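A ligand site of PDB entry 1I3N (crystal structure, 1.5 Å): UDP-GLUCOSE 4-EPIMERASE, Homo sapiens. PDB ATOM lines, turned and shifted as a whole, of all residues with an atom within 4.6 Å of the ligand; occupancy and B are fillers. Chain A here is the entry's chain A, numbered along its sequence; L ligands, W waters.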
ATOM      1  N   LYS A  92      12.175  31.120 -31.166  1.00  0.00           N
ATOM      2  CA  LYS A  92      12.305  30.119 -30.142  1.00  0.00           C
ATOM      3  C   LYS A  92      11.007  30.176 -29.378  1.00  0.00           C
ATOM      4  O   LYS A  92      10.230  31.111 -29.530  1.00  0.00           O
ATOM      5  CB  LYS A  92      13.560  30.113 -29.277  1.00  0.00           C
ATOM      6  CG  LYS A  92      14.258  31.434 -29.093  1.00  0.00           C
ATOM      7  CD  LYS A  92      15.216  31.381 -27.925  1.00  0.00           C
ATOM      8  CE  LYS A  92      15.169  32.608 -27.048  1.00  0.00           C
ATOM      9  NZ  LYS A  92      16.252  32.626 -26.064  1.00  0.00           N
ATOM     10  N   ALA A  93      10.687  29.165 -28.626  1.00  0.00           N
ATOM     11  CA  ALA A  93       9.420  29.338 -28.008  1.00  0.00           C
ATOM     12  C   ALA A  93       9.508  30.007 -26.671  1.00  0.00           C
ATOM     13  O   ALA A  93      10.431  29.760 -25.894  1.00  0.00           O
ATOM     14  CB  ALA A  93       8.501  28.154 -28.110  1.00  0.00           C
ATOM     15  N   THR A 134      16.060  19.651 -27.622  1.00  0.00           N
ATOM     16  CA  THR A 134      14.630  19.340 -27.731  1.00  0.00           C
ATOM     17  C   THR A 134      14.357  18.347 -28.831  1.00  0.00           C
ATOM     18  O   THR A 134      13.327  17.672 -28.830  1.00  0.00           O
ATOM     19  CB  THR A 134      13.719  20.580 -27.988  1.00  0.00           C
ATOM     20  OG1 THR A 134      14.167  21.237 -29.163  1.00  0.00           O
ATOM     21  CG2 THR A 134      13.746  21.509 -26.785  1.00  0.00           C
ATOM     22  N   ASN A 155       6.447  19.920 -29.540  1.00  0.00           N
ATOM     23  CA  ASN A 155       6.068  21.139 -30.226  1.00  0.00           C
ATOM     24  C   ASN A 155       6.621  21.493 -31.604  1.00  0.00           C
ATOM     25  O   ASN A 155       7.607  20.943 -32.093  1.00  0.00           O
ATOM     26  CB  ASN A 155       6.275  22.331 -29.266  1.00  0.00           C
ATOM     27  CG  ASN A 155       7.708  22.481 -28.768  1.00  0.00           C
ATOM     28  OD1 ASN A 155       8.619  22.877 -29.497  1.00  0.00           O
ATOM     29  ND2 ASN A 155       7.898  22.120 -27.517  1.00  0.00           N
ATOM     30  N   TYR A 157       8.157  24.117 -32.367  1.00  0.00           N
ATOM     31  CA  TYR A 157       9.500  24.638 -32.329  1.00  0.00           C
ATOM     32  C   TYR A 157      10.533  23.497 -32.467  1.00  0.00           C
ATOM     33  O   TYR A 157      11.450  23.558 -33.268  1.00  0.00           O
ATOM     34  CB  TYR A 157       9.759  25.430 -31.028  1.00  0.00           C
ATOM     35  CG  TYR A 157      11.245  25.662 -30.775  1.00  0.00           C
ATOM     36  CD1 TYR A 157      11.947  24.924 -29.813  1.00  0.00           C
ATOM     37  CD2 TYR A 157      11.974  26.584 -31.531  1.00  0.00           C
ATOM     38  CE1 TYR A 157      13.315  25.125 -29.598  1.00  0.00           C
ATOM     39  CE2 TYR A 157      13.330  26.813 -31.339  1.00  0.00           C
ATOM     40  CZ  TYR A 157      14.000  26.094 -30.348  1.00  0.00           C
ATOM     41  OH  TYR A 157      15.337  26.312 -30.144  1.00  0.00           O
ATOM     42  N   ASN A 187      21.009  23.832 -22.066  1.00  0.00           N
ATOM     43  CA  ASN A 187      20.352  25.033 -21.520  1.00  0.00           C
ATOM     44  C   ASN A 187      21.346  26.160 -21.285  1.00  0.00           C
ATOM     45  O   ASN A 187      21.972  26.245 -20.225  1.00  0.00           O
ATOM     46  CB  ASN A 187      19.565  24.717 -20.234  1.00  0.00           C
ATOM     47  CG  ASN A 187      18.328  23.871 -20.504  1.00  0.00           C
ATOM     48  OD1 ASN A 187      18.437  22.747 -21.026  1.00  0.00           O
ATOM     49  ND2 ASN A 187      17.155  24.377 -20.174  1.00  0.00           N
ATOM     50  N   ASN A 206      10.275  33.425 -19.747  1.00  0.00           N
ATOM     51  CA  ASN A 206       9.719  32.101 -19.810  1.00  0.00           C
ATOM     52  C   ASN A 206      10.726  31.051 -19.341  1.00  0.00           C
ATOM     53  O   ASN A 206      10.351  29.959 -18.895  1.00  0.00           O
ATOM     54  CB  ASN A 206       9.140  31.791 -21.208  1.00  0.00           C
ATOM     55  CG  ASN A 206       8.181  32.865 -21.677  1.00  0.00           C
ATOM     56  OD1 ASN A 206       8.552  33.746 -22.493  1.00  0.00           O
ATOM     57  ND2 ASN A 206       6.963  32.807 -21.137  1.00  0.00           N
ATOM     58  N   ASN A 207      12.003  31.390 -19.415  1.00  0.00           N
ATOM     59  CA  ASN A 207      13.067  30.501 -19.005  1.00  0.00           C
ATOM     60  C   ASN A 207      13.441  30.727 -17.563  1.00  0.00           C
ATOM     61  O   ASN A 207      13.219  31.755 -16.967  1.00  0.00           O
ATOM     62  CB  ASN A 207      14.243  30.453 -19.990  1.00  0.00           C
ATOM     63  CG  ASN A 207      14.890  31.786 -20.267  1.00  0.00           C
ATOM     64  OD1 ASN A 207      14.223  32.845 -20.324  1.00  0.00           O
ATOM     65  ND2 ASN A 207      16.218  31.732 -20.450  1.00  0.00           N
ATOM     66  N   LEU A 208      13.994  29.709 -16.947  1.00  0.00           N
ATOM     67  CA  LEU A 208      14.303  29.757 -15.537  1.00  0.00           C
ATOM     68  C   LEU A 208      15.261  30.824 -15.029  1.00  0.00           C
ATOM     69  O   LEU A 208      14.938  31.617 -14.160  1.00  0.00           O
ATOM     70  CB  LEU A 208      14.874  28.380 -15.083  1.00  0.00           C
ATOM     71  CG  LEU A 208      15.252  28.316 -13.606  1.00  0.00           C
ATOM     72  CD1 LEU A 208      14.016  28.475 -12.727  1.00  0.00           C
ATOM     73  CD2 LEU A 208      15.931  26.967 -13.354  1.00  0.00           C
ATOM     74  N   TYR A 211      14.436  34.517 -14.813  1.00  0.00           N
ATOM     75  CA  TYR A 211      13.405  34.757 -13.828  1.00  0.00           C
ATOM     76  C   TYR A 211      14.077  34.772 -12.455  1.00  0.00           C
ATOM     77  O   TYR A 211      13.866  35.662 -11.630  1.00  0.00           O
ATOM     78  CB  TYR A 211      12.249  33.775 -13.941  1.00  0.00           C
ATOM     79  CG  TYR A 211      10.962  34.316 -13.352  1.00  0.00           C
ATOM     80  CD1 TYR A 211      10.803  34.436 -11.977  1.00  0.00           C
ATOM     81  CD2 TYR A 211       9.881  34.659 -14.175  1.00  0.00           C
ATOM     82  CE1 TYR A 211       9.612  34.914 -11.405  1.00  0.00           C
ATOM     83  CE2 TYR A 211       8.680  35.134 -13.633  1.00  0.00           C
ATOM     84  CZ  TYR A 211       8.549  35.277 -12.249  1.00  0.00           C
ATOM     85  OH  TYR A 211       7.407  35.769 -11.657  1.00  0.00           O
ATOM     86  N   LEU A 223       9.988  33.142  -7.256  1.00  0.00           N
ATOM     87  CA  LEU A 223      10.066  32.274  -8.412  1.00  0.00           C
ATOM     88  C   LEU A 223       8.889  31.308  -8.366  1.00  0.00           C
ATOM     89  O   LEU A 223       8.539  30.803  -7.309  1.00  0.00           O
ATOM     90  CB  LEU A 223      11.385  31.453  -8.435  1.00  0.00           C
ATOM     91  CG  LEU A 223      11.340  30.244  -9.404  1.00  0.00           C
ATOM     92  CD1 LEU A 223      11.573  30.699 -10.859  1.00  0.00           C
ATOM     93  CD2 LEU A 223      12.432  29.254  -9.058  1.00  0.00           C
ATOM     94  N   ASN A 224       8.255  31.067  -9.517  1.00  0.00           N
ATOM     95  CA  ASN A 224       7.198  30.105  -9.590  1.00  0.00           C
ATOM     96  C   ASN A 224       7.861  28.828 -10.042  1.00  0.00           C
ATOM     97  O   ASN A 224       8.404  28.794 -11.130  1.00  0.00           O
ATOM     98  CB  ASN A 224       6.082  30.506 -10.586  1.00  0.00           C
ATOM     99  CG  ASN A 224       5.417  31.801 -10.175  1.00  0.00           C
ATOM    100  OD1 ASN A 224       5.289  32.775 -10.947  1.00  0.00           O
ATOM    101  ND2 ASN A 224       5.033  31.846  -8.917  1.00  0.00           N
ATOM    102  N   VAL A 225       7.863  27.807  -9.208  1.00  0.00           N
ATOM    103  CA  VAL A 225       8.485  26.542  -9.561  1.00  0.00           C
ATOM    104  C   VAL A 225       7.409  25.678 -10.230  1.00  0.00           C
ATOM    105  O   VAL A 225       6.371  25.365  -9.647  1.00  0.00           O
ATOM    106  CB  VAL A 225       9.139  25.895  -8.333  1.00  0.00           C
ATOM    107  CG1 VAL A 225       9.535  24.444  -8.637  1.00  0.00           C
ATOM    108  CG2 VAL A 225      10.349  26.699  -7.871  1.00  0.00           C
ATOM    109  N   PHE A 226       7.650  25.291 -11.481  1.00  0.00           N
ATOM    110  CA  PHE A 226       6.679  24.500 -12.254  1.00  0.00           C
ATOM    111  C   PHE A 226       6.656  23.029 -11.917  1.00  0.00           C
ATOM    112  O   PHE A 226       7.132  22.202 -12.694  1.00  0.00           O
ATOM    113  CB  PHE A 226       6.939  24.622 -13.772  1.00  0.00           C
ATOM    114  CG  PHE A 226       6.936  26.031 -14.296  1.00  0.00           C
ATOM    115  CD1 PHE A 226       7.631  26.366 -15.462  1.00  0.00           C
ATOM    116  CD2 PHE A 226       6.235  27.035 -13.609  1.00  0.00           C
ATOM    117  CE1 PHE A 226       7.626  27.676 -15.951  1.00  0.00           C
ATOM    118  CE2 PHE A 226       6.221  28.345 -14.088  1.00  0.00           C
ATOM    119  CZ  PHE A 226       6.917  28.661 -15.254  1.00  0.00           C
ATOM    120  N   GLY A 237      12.462  19.774 -11.929  1.00  0.00           N
ATOM    121  CA  GLY A 237      13.127  19.479 -13.193  1.00  0.00           C
ATOM    122  C   GLY A 237      14.629  19.642 -13.136  1.00  0.00           C
ATOM    123  O   GLY A 237      15.179  20.543 -12.501  1.00  0.00           O
ATOM    124  N   ARG A 239      18.140  19.868 -15.500  1.00  0.00           N
ATOM    125  CA  ARG A 239      18.658  20.274 -16.801  1.00  0.00           C
ATOM    126  C   ARG A 239      20.157  20.474 -16.797  1.00  0.00           C
ATOM    127  O   ARG A 239      20.766  20.767 -15.768  1.00  0.00           O
ATOM    128  CB  ARG A 239      18.041  21.597 -17.253  1.00  0.00           C
ATOM    129  CG  ARG A 239      16.514  21.614 -17.289  1.00  0.00           C
ATOM    130  CD  ARG A 239      15.983  20.836 -18.491  1.00  0.00           C
ATOM    131  NE  ARG A 239      14.543  20.915 -18.630  1.00  0.00           N
ATOM    132  CZ  ARG A 239      13.634  20.108 -18.081  1.00  0.00           C
ATOM    133  NH1 ARG A 239      13.936  19.098 -17.296  1.00  0.00           N
ATOM    134  NH2 ARG A 239      12.361  20.344 -18.348  1.00  0.00           N
ATOM    135  N   TYR A 241      22.745  22.860 -17.563  1.00  0.00           N
ATOM    136  CA  TYR A 241      22.992  24.293 -17.797  1.00  0.00           C
ATOM    137  C   TYR A 241      24.400  24.491 -18.284  1.00  0.00           C
ATOM    138  O   TYR A 241      25.328  23.932 -17.711  1.00  0.00           O
ATOM    139  CB  TYR A 241      22.697  25.110 -16.529  1.00  0.00           C
ATOM    140  CG  TYR A 241      21.231  25.011 -16.178  1.00  0.00           C
ATOM    141  CD1 TYR A 241      20.274  25.805 -16.834  1.00  0.00           C
ATOM    142  CD2 TYR A 241      20.771  24.121 -15.212  1.00  0.00           C
ATOM    143  CE1 TYR A 241      18.917  25.712 -16.543  1.00  0.00           C
ATOM    144  CE2 TYR A 241      19.406  24.009 -14.900  1.00  0.00           C
ATOM    145  CZ  TYR A 241      18.478  24.814 -15.576  1.00  0.00           C
ATOM    146  OH  TYR A 241      17.143  24.701 -15.304  1.00  0.00           O
ATOM    147  N   VAL A 277      15.919  22.620 -10.403  1.00  0.00           N
ATOM    148  CA  VAL A 277      15.430  23.976 -10.245  1.00  0.00           C
ATOM    149  C   VAL A 277      15.909  24.526  -8.901  1.00  0.00           C
ATOM    150  O   VAL A 277      16.516  25.595  -8.794  1.00  0.00           O
ATOM    151  CB  VAL A 277      13.904  23.988 -10.381  1.00  0.00           C
ATOM    152  CG1 VAL A 277      13.332  25.376 -10.045  1.00  0.00           C
ATOM    153  CG2 VAL A 277      13.469  23.508 -11.780  1.00  0.00           C
ATOM    154  N   ARG A 300       4.300  22.589 -15.968  1.00  0.00           N
ATOM    155  CA  ARG A 300       4.182  23.297 -17.227  1.00  0.00           C
ATOM    156  C   ARG A 300       3.962  22.269 -18.295  1.00  0.00           C
ATOM    157  O   ARG A 300       4.692  21.290 -18.352  1.00  0.00           O
ATOM    158  CB  ARG A 300       5.476  24.048 -17.512  1.00  0.00           C
ATOM    159  CG  ARG A 300       5.401  24.848 -18.805  1.00  0.00           C
ATOM    160  CD  ARG A 300       6.601  25.781 -18.930  1.00  0.00           C
ATOM    161  NE  ARG A 300       7.917  25.131 -18.962  1.00  0.00           N
ATOM    162  CZ  ARG A 300       9.111  25.755 -19.031  1.00  0.00           C
ATOM    163  NH1 ARG A 300       9.216  27.083 -18.959  1.00  0.00           N
ATOM    164  NH2 ARG A 300      10.222  25.026 -19.109  1.00  0.00           N
ATOM    165  N   GLU A 301       2.950  22.496 -19.131  1.00  0.00           N
ATOM    166  CA  GLU A 301       2.653  21.553 -20.205  1.00  0.00           C
ATOM    167  C   GLU A 301       3.875  21.184 -21.043  1.00  0.00           C
ATOM    168  O   GLU A 301       4.588  22.059 -21.537  1.00  0.00           O
ATOM    169  CB  GLU A 301       1.490  22.046 -21.106  1.00  0.00           C
ATOM    170  CG  GLU A 301       1.749  21.917 -22.620  1.00  0.00           C
ATOM    171  CD  GLU A 301       0.703  22.580 -23.509  1.00  0.00           C
ATOM    172  OE1 GLU A 301      -0.488  22.293 -23.548  1.00  0.00           O
ATOM    173  OE2 GLU A 301       1.219  23.526 -24.278  1.00  0.00           O
ATOM    174  N   GLY A 302       4.100  19.870 -21.164  1.00  0.00           N
ATOM    175  CA  GLY A 302       5.189  19.292 -21.961  1.00  0.00           C
ATOM    176  C   GLY A 302       6.595  19.274 -21.385  1.00  0.00           C
ATOM    177  O   GLY A 302       7.525  18.928 -22.105  1.00  0.00           O
ATOM    178  N   ASP A 303       6.735  19.672 -20.123  1.00  0.00           N
ATOM    179  CA  ASP A 303       8.005  19.729 -19.441  1.00  0.00           C
ATOM    180  C   ASP A 303       8.527  18.347 -19.187  1.00  0.00           C
ATOM    181  O   ASP A 303       7.732  17.503 -18.745  1.00  0.00           O
ATOM    182  CB  ASP A 303       7.781  20.425 -18.086  1.00  0.00           C
ATOM    183  CG  ASP A 303       8.532  21.693 -18.020  1.00  0.00           C
ATOM    184  OD1 ASP A 303       9.341  21.984 -18.883  1.00  0.00           O
ATOM    185  OD2 ASP A 303       8.275  22.422 -16.957  1.00  0.00           O
ATOM    186  N   VAL A 304       9.820  18.105 -19.441  1.00  0.00           N
ATOM    187  CA  VAL A 304      10.376  16.799 -19.151  1.00  0.00           C
ATOM    188  C   VAL A 304      10.920  16.785 -17.746  1.00  0.00           C
ATOM    189  O   VAL A 304      11.219  17.814 -17.158  1.00  0.00           O
ATOM    190  CB  VAL A 304      11.364  16.221 -20.169  1.00  0.00           C
ATOM    191  CG1 VAL A 304      10.992  16.589 -21.601  1.00  0.00           C
ATOM    192  CG2 VAL A 304      12.774  16.651 -19.856  1.00  0.00           C
HETATM  193  C1  LIG L   1      12.839  23.866 -23.176  1.00  0.00           C
HETATM  194  C2  LIG L   1      11.943  24.659 -24.121  1.00  0.00           C
HETATM  195  C3  LIG L   1      10.496  24.569 -23.641  1.00  0.00           C
HETATM  196  C4  LIG L   1      10.068  23.132 -23.387  1.00  0.00           C
HETATM  197  C5  LIG L   1      11.069  22.424 -22.516  1.00  0.00           C
HETATM  198  C6  LIG L   1      10.715  20.950 -22.300  1.00  0.00           C
HETATM  199  C7  LIG L   1      13.135  26.426 -25.191  1.00  0.00           C
HETATM  200  C8  LIG L   1      13.492  27.868 -25.445  1.00  0.00           C
HETATM  201  N1  LIG L   1      12.330  26.093 -24.185  1.00  0.00           N
HETATM  202  O1  LIG L   1      12.627  24.399 -21.892  1.00  0.00           O
HETATM  203  O2  LIG L   1       9.629  25.111 -24.643  1.00  0.00           O
HETATM  204  O3  LIG L   1       8.775  23.000 -22.784  1.00  0.00           O
HETATM  205  O4  LIG L   1      12.355  22.512 -23.167  1.00  0.00           O
HETATM  206  O5  LIG L   1      10.576  20.281 -23.557  1.00  0.00           O
HETATM  207  O6  LIG L   1      13.614  25.573 -25.906  1.00  0.00           O
HETATM  208  N2  LIG L   1      11.132  26.500 -14.597  1.00  0.00           N
HETATM  209  C9  LIG L   1      10.364  26.828 -13.485  1.00  0.00           C
HETATM  210  N3  LIG L   1       9.911  28.118 -13.483  1.00  0.00           N
HETATM  211  C10 LIG L   1      10.133  29.099 -14.465  1.00  0.00           C
HETATM  212  C11 LIG L   1      10.919  28.662 -15.561  1.00  0.00           C
HETATM  213  C12 LIG L   1      11.378  27.431 -15.596  1.00  0.00           C
HETATM  214  O7  LIG L   1      10.104  26.073 -12.555  1.00  0.00           O
HETATM  215  O8  LIG L   1       9.653  30.213 -14.324  1.00  0.00           O
HETATM  216  C13 LIG L   1      11.731  25.155 -14.715  1.00  0.00           C
HETATM  217  C14 LIG L   1      11.226  24.302 -15.854  1.00  0.00           C
HETATM  218  O9  LIG L   1      10.061  23.557 -15.458  1.00  0.00           O
HETATM  219  C15 LIG L   1      12.416  23.339 -16.090  1.00  0.00           C
HETATM  220  C16 LIG L   1      13.598  24.243 -15.783  1.00  0.00           C
HETATM  221  O10 LIG L   1      13.107  25.257 -14.856  1.00  0.00           O
HETATM  222  O11 LIG L   1      12.409  22.167 -15.258  1.00  0.00           O
HETATM  223  C17 LIG L   1      14.196  24.911 -16.987  1.00  0.00           C
HETATM  224  O12 LIG L   1      13.088  25.457 -17.730  1.00  0.00           O
HETATM  225  P1  LIG L   1      13.415  26.381 -18.989  1.00  0.00           P
HETATM  226  O13 LIG L   1      12.167  26.925 -19.562  1.00  0.00           O
HETATM  227  O14 LIG L   1      14.449  27.384 -18.677  1.00  0.00           O
HETATM  228  O15 LIG L   1      14.133  25.291 -20.001  1.00  0.00           O
HETATM  229  P2  LIG L   1      13.575  23.978 -20.626  1.00  0.00           P
HETATM  230  O16 LIG L   1      14.778  23.219 -21.033  1.00  0.00           O
HETATM  231  O17 LIG L   1      12.701  23.245 -19.679  1.00  0.00           O
HETATM  232  O   HOH W   1       7.358  22.426 -20.846  1.00  0.00           O
HETATM  233  O   HOH W   2      17.069  27.221 -19.451  1.00  0.00           O
HETATM  234  O   HOH W   3      15.270  30.238 -23.940  1.00  0.00           O
HETATM  235  O   HOH W   4      15.925  26.307 -23.263  1.00  0.00           O
HETATM  236  O   HOH W   5      11.309  27.973 -22.033  1.00  0.00           O
HETATM  237  O   HOH W   6       8.544  31.768 -16.332  1.00  0.00           O
HETATM  238  O   HOH W   7       8.554  31.936 -12.375  1.00  0.00           O
HETATM  239  O   HOH W   8      11.048  17.864 -25.533  1.00  0.00           O
HETATM  240  O   HOH W   9      10.425  19.993 -15.382  1.00  0.00           O
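The side-chain carboxylate (OD2) of Asp 303 sits at hydrogen-bond distance from an oxygen (O9) of the ligand, at 2.6 Å.
O13 of the ligand lies within salt-bridge range of NH2 of Arg 300, 2.8 Å away.
The side-chain amide nitrogen of Asn 187 is in hydrogen-bond range of an oxygen (O16) of the ligand (2.8 Å).
An oxygen (O7) of the ligand sits at hydrogen-bond distance from the backbone NH (N) of Phe 226, 2.8 Å away.
The backbone carbonyl oxygen (O) of Asn 224 is in hydrogen-bond range of a nitrogen (N3) of the ligand, 2.9 Å away.
An oxygen (O14) of the ligand sits at hydrogen-bond distance from the backbone NH of Leu 208 (2.9 Å).
The guanidinium group (NE) of Arg 239 is in salt-bridge range of an oxygen (O17) of the ligand (3.1 Å).
The side-chain carboxylate (OD1) of Asp 303 is in salt-bridge range of the guanidinium group (NH2) of Arg 300, 3.2 Å away.
OD1 of Asp 303 is in salt-bridge range of NH2 of Arg 239 (3.5 Å).
The guanidinium group (NH1) of Arg 300 sits at hydrogen-bond distance from the backbone carbonyl oxygen (O) of Asn 206 (3.1 Å).
NH1 of Arg 239 lies within hydrogen-bond range of O of Val 304.
The backbone carbonyl oxygen (O) of Gly 237 lies within hydrogen-bond range of the backbone NH (N) of Val 277, at 3.0 Å.
The backbone NH (N) of Tyr 157 lies close to the side-chain amide oxygen (OD1) of Asn 155, 3.2 Å away.
Residues that only touch the ligand: Ala 93, Tyr 157, Asn 206, Asn 207, Leu 223, Val 225, Gly 237, Tyr 241, Val 277 and Gly 302.
Hydrophobic or aromatic side chains within 4 Å of the ligand: Tyr 157, Leu 208, Leu 223, Phe 226 and Val 277.
Of the 23 residues printed, 17 come within 4 Å of the ligand.
Water W1 lies within hydrogen-bond range of an oxygen (O3) of the ligand (2.5 Å), the side-chain carboxylate of Asp 303 (2.8 Å), the backbone carbonyl oxygen of Glu 301 (2.9 Å) and the guanidinium group of Arg 300 (3.3 Å).
Water W2 bridges an oxygen (O14) of the ligand and the side-chain amide nitrogen of Asn 187.
Water W7 bridges an oxygen (O8) of the ligand (2.8 Å) and the backbone NH (N) of Asn 224 (3.0 Å).
Water W9 lies within hydrogen-bond range of O of Val 304 and O11 of the ligand.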
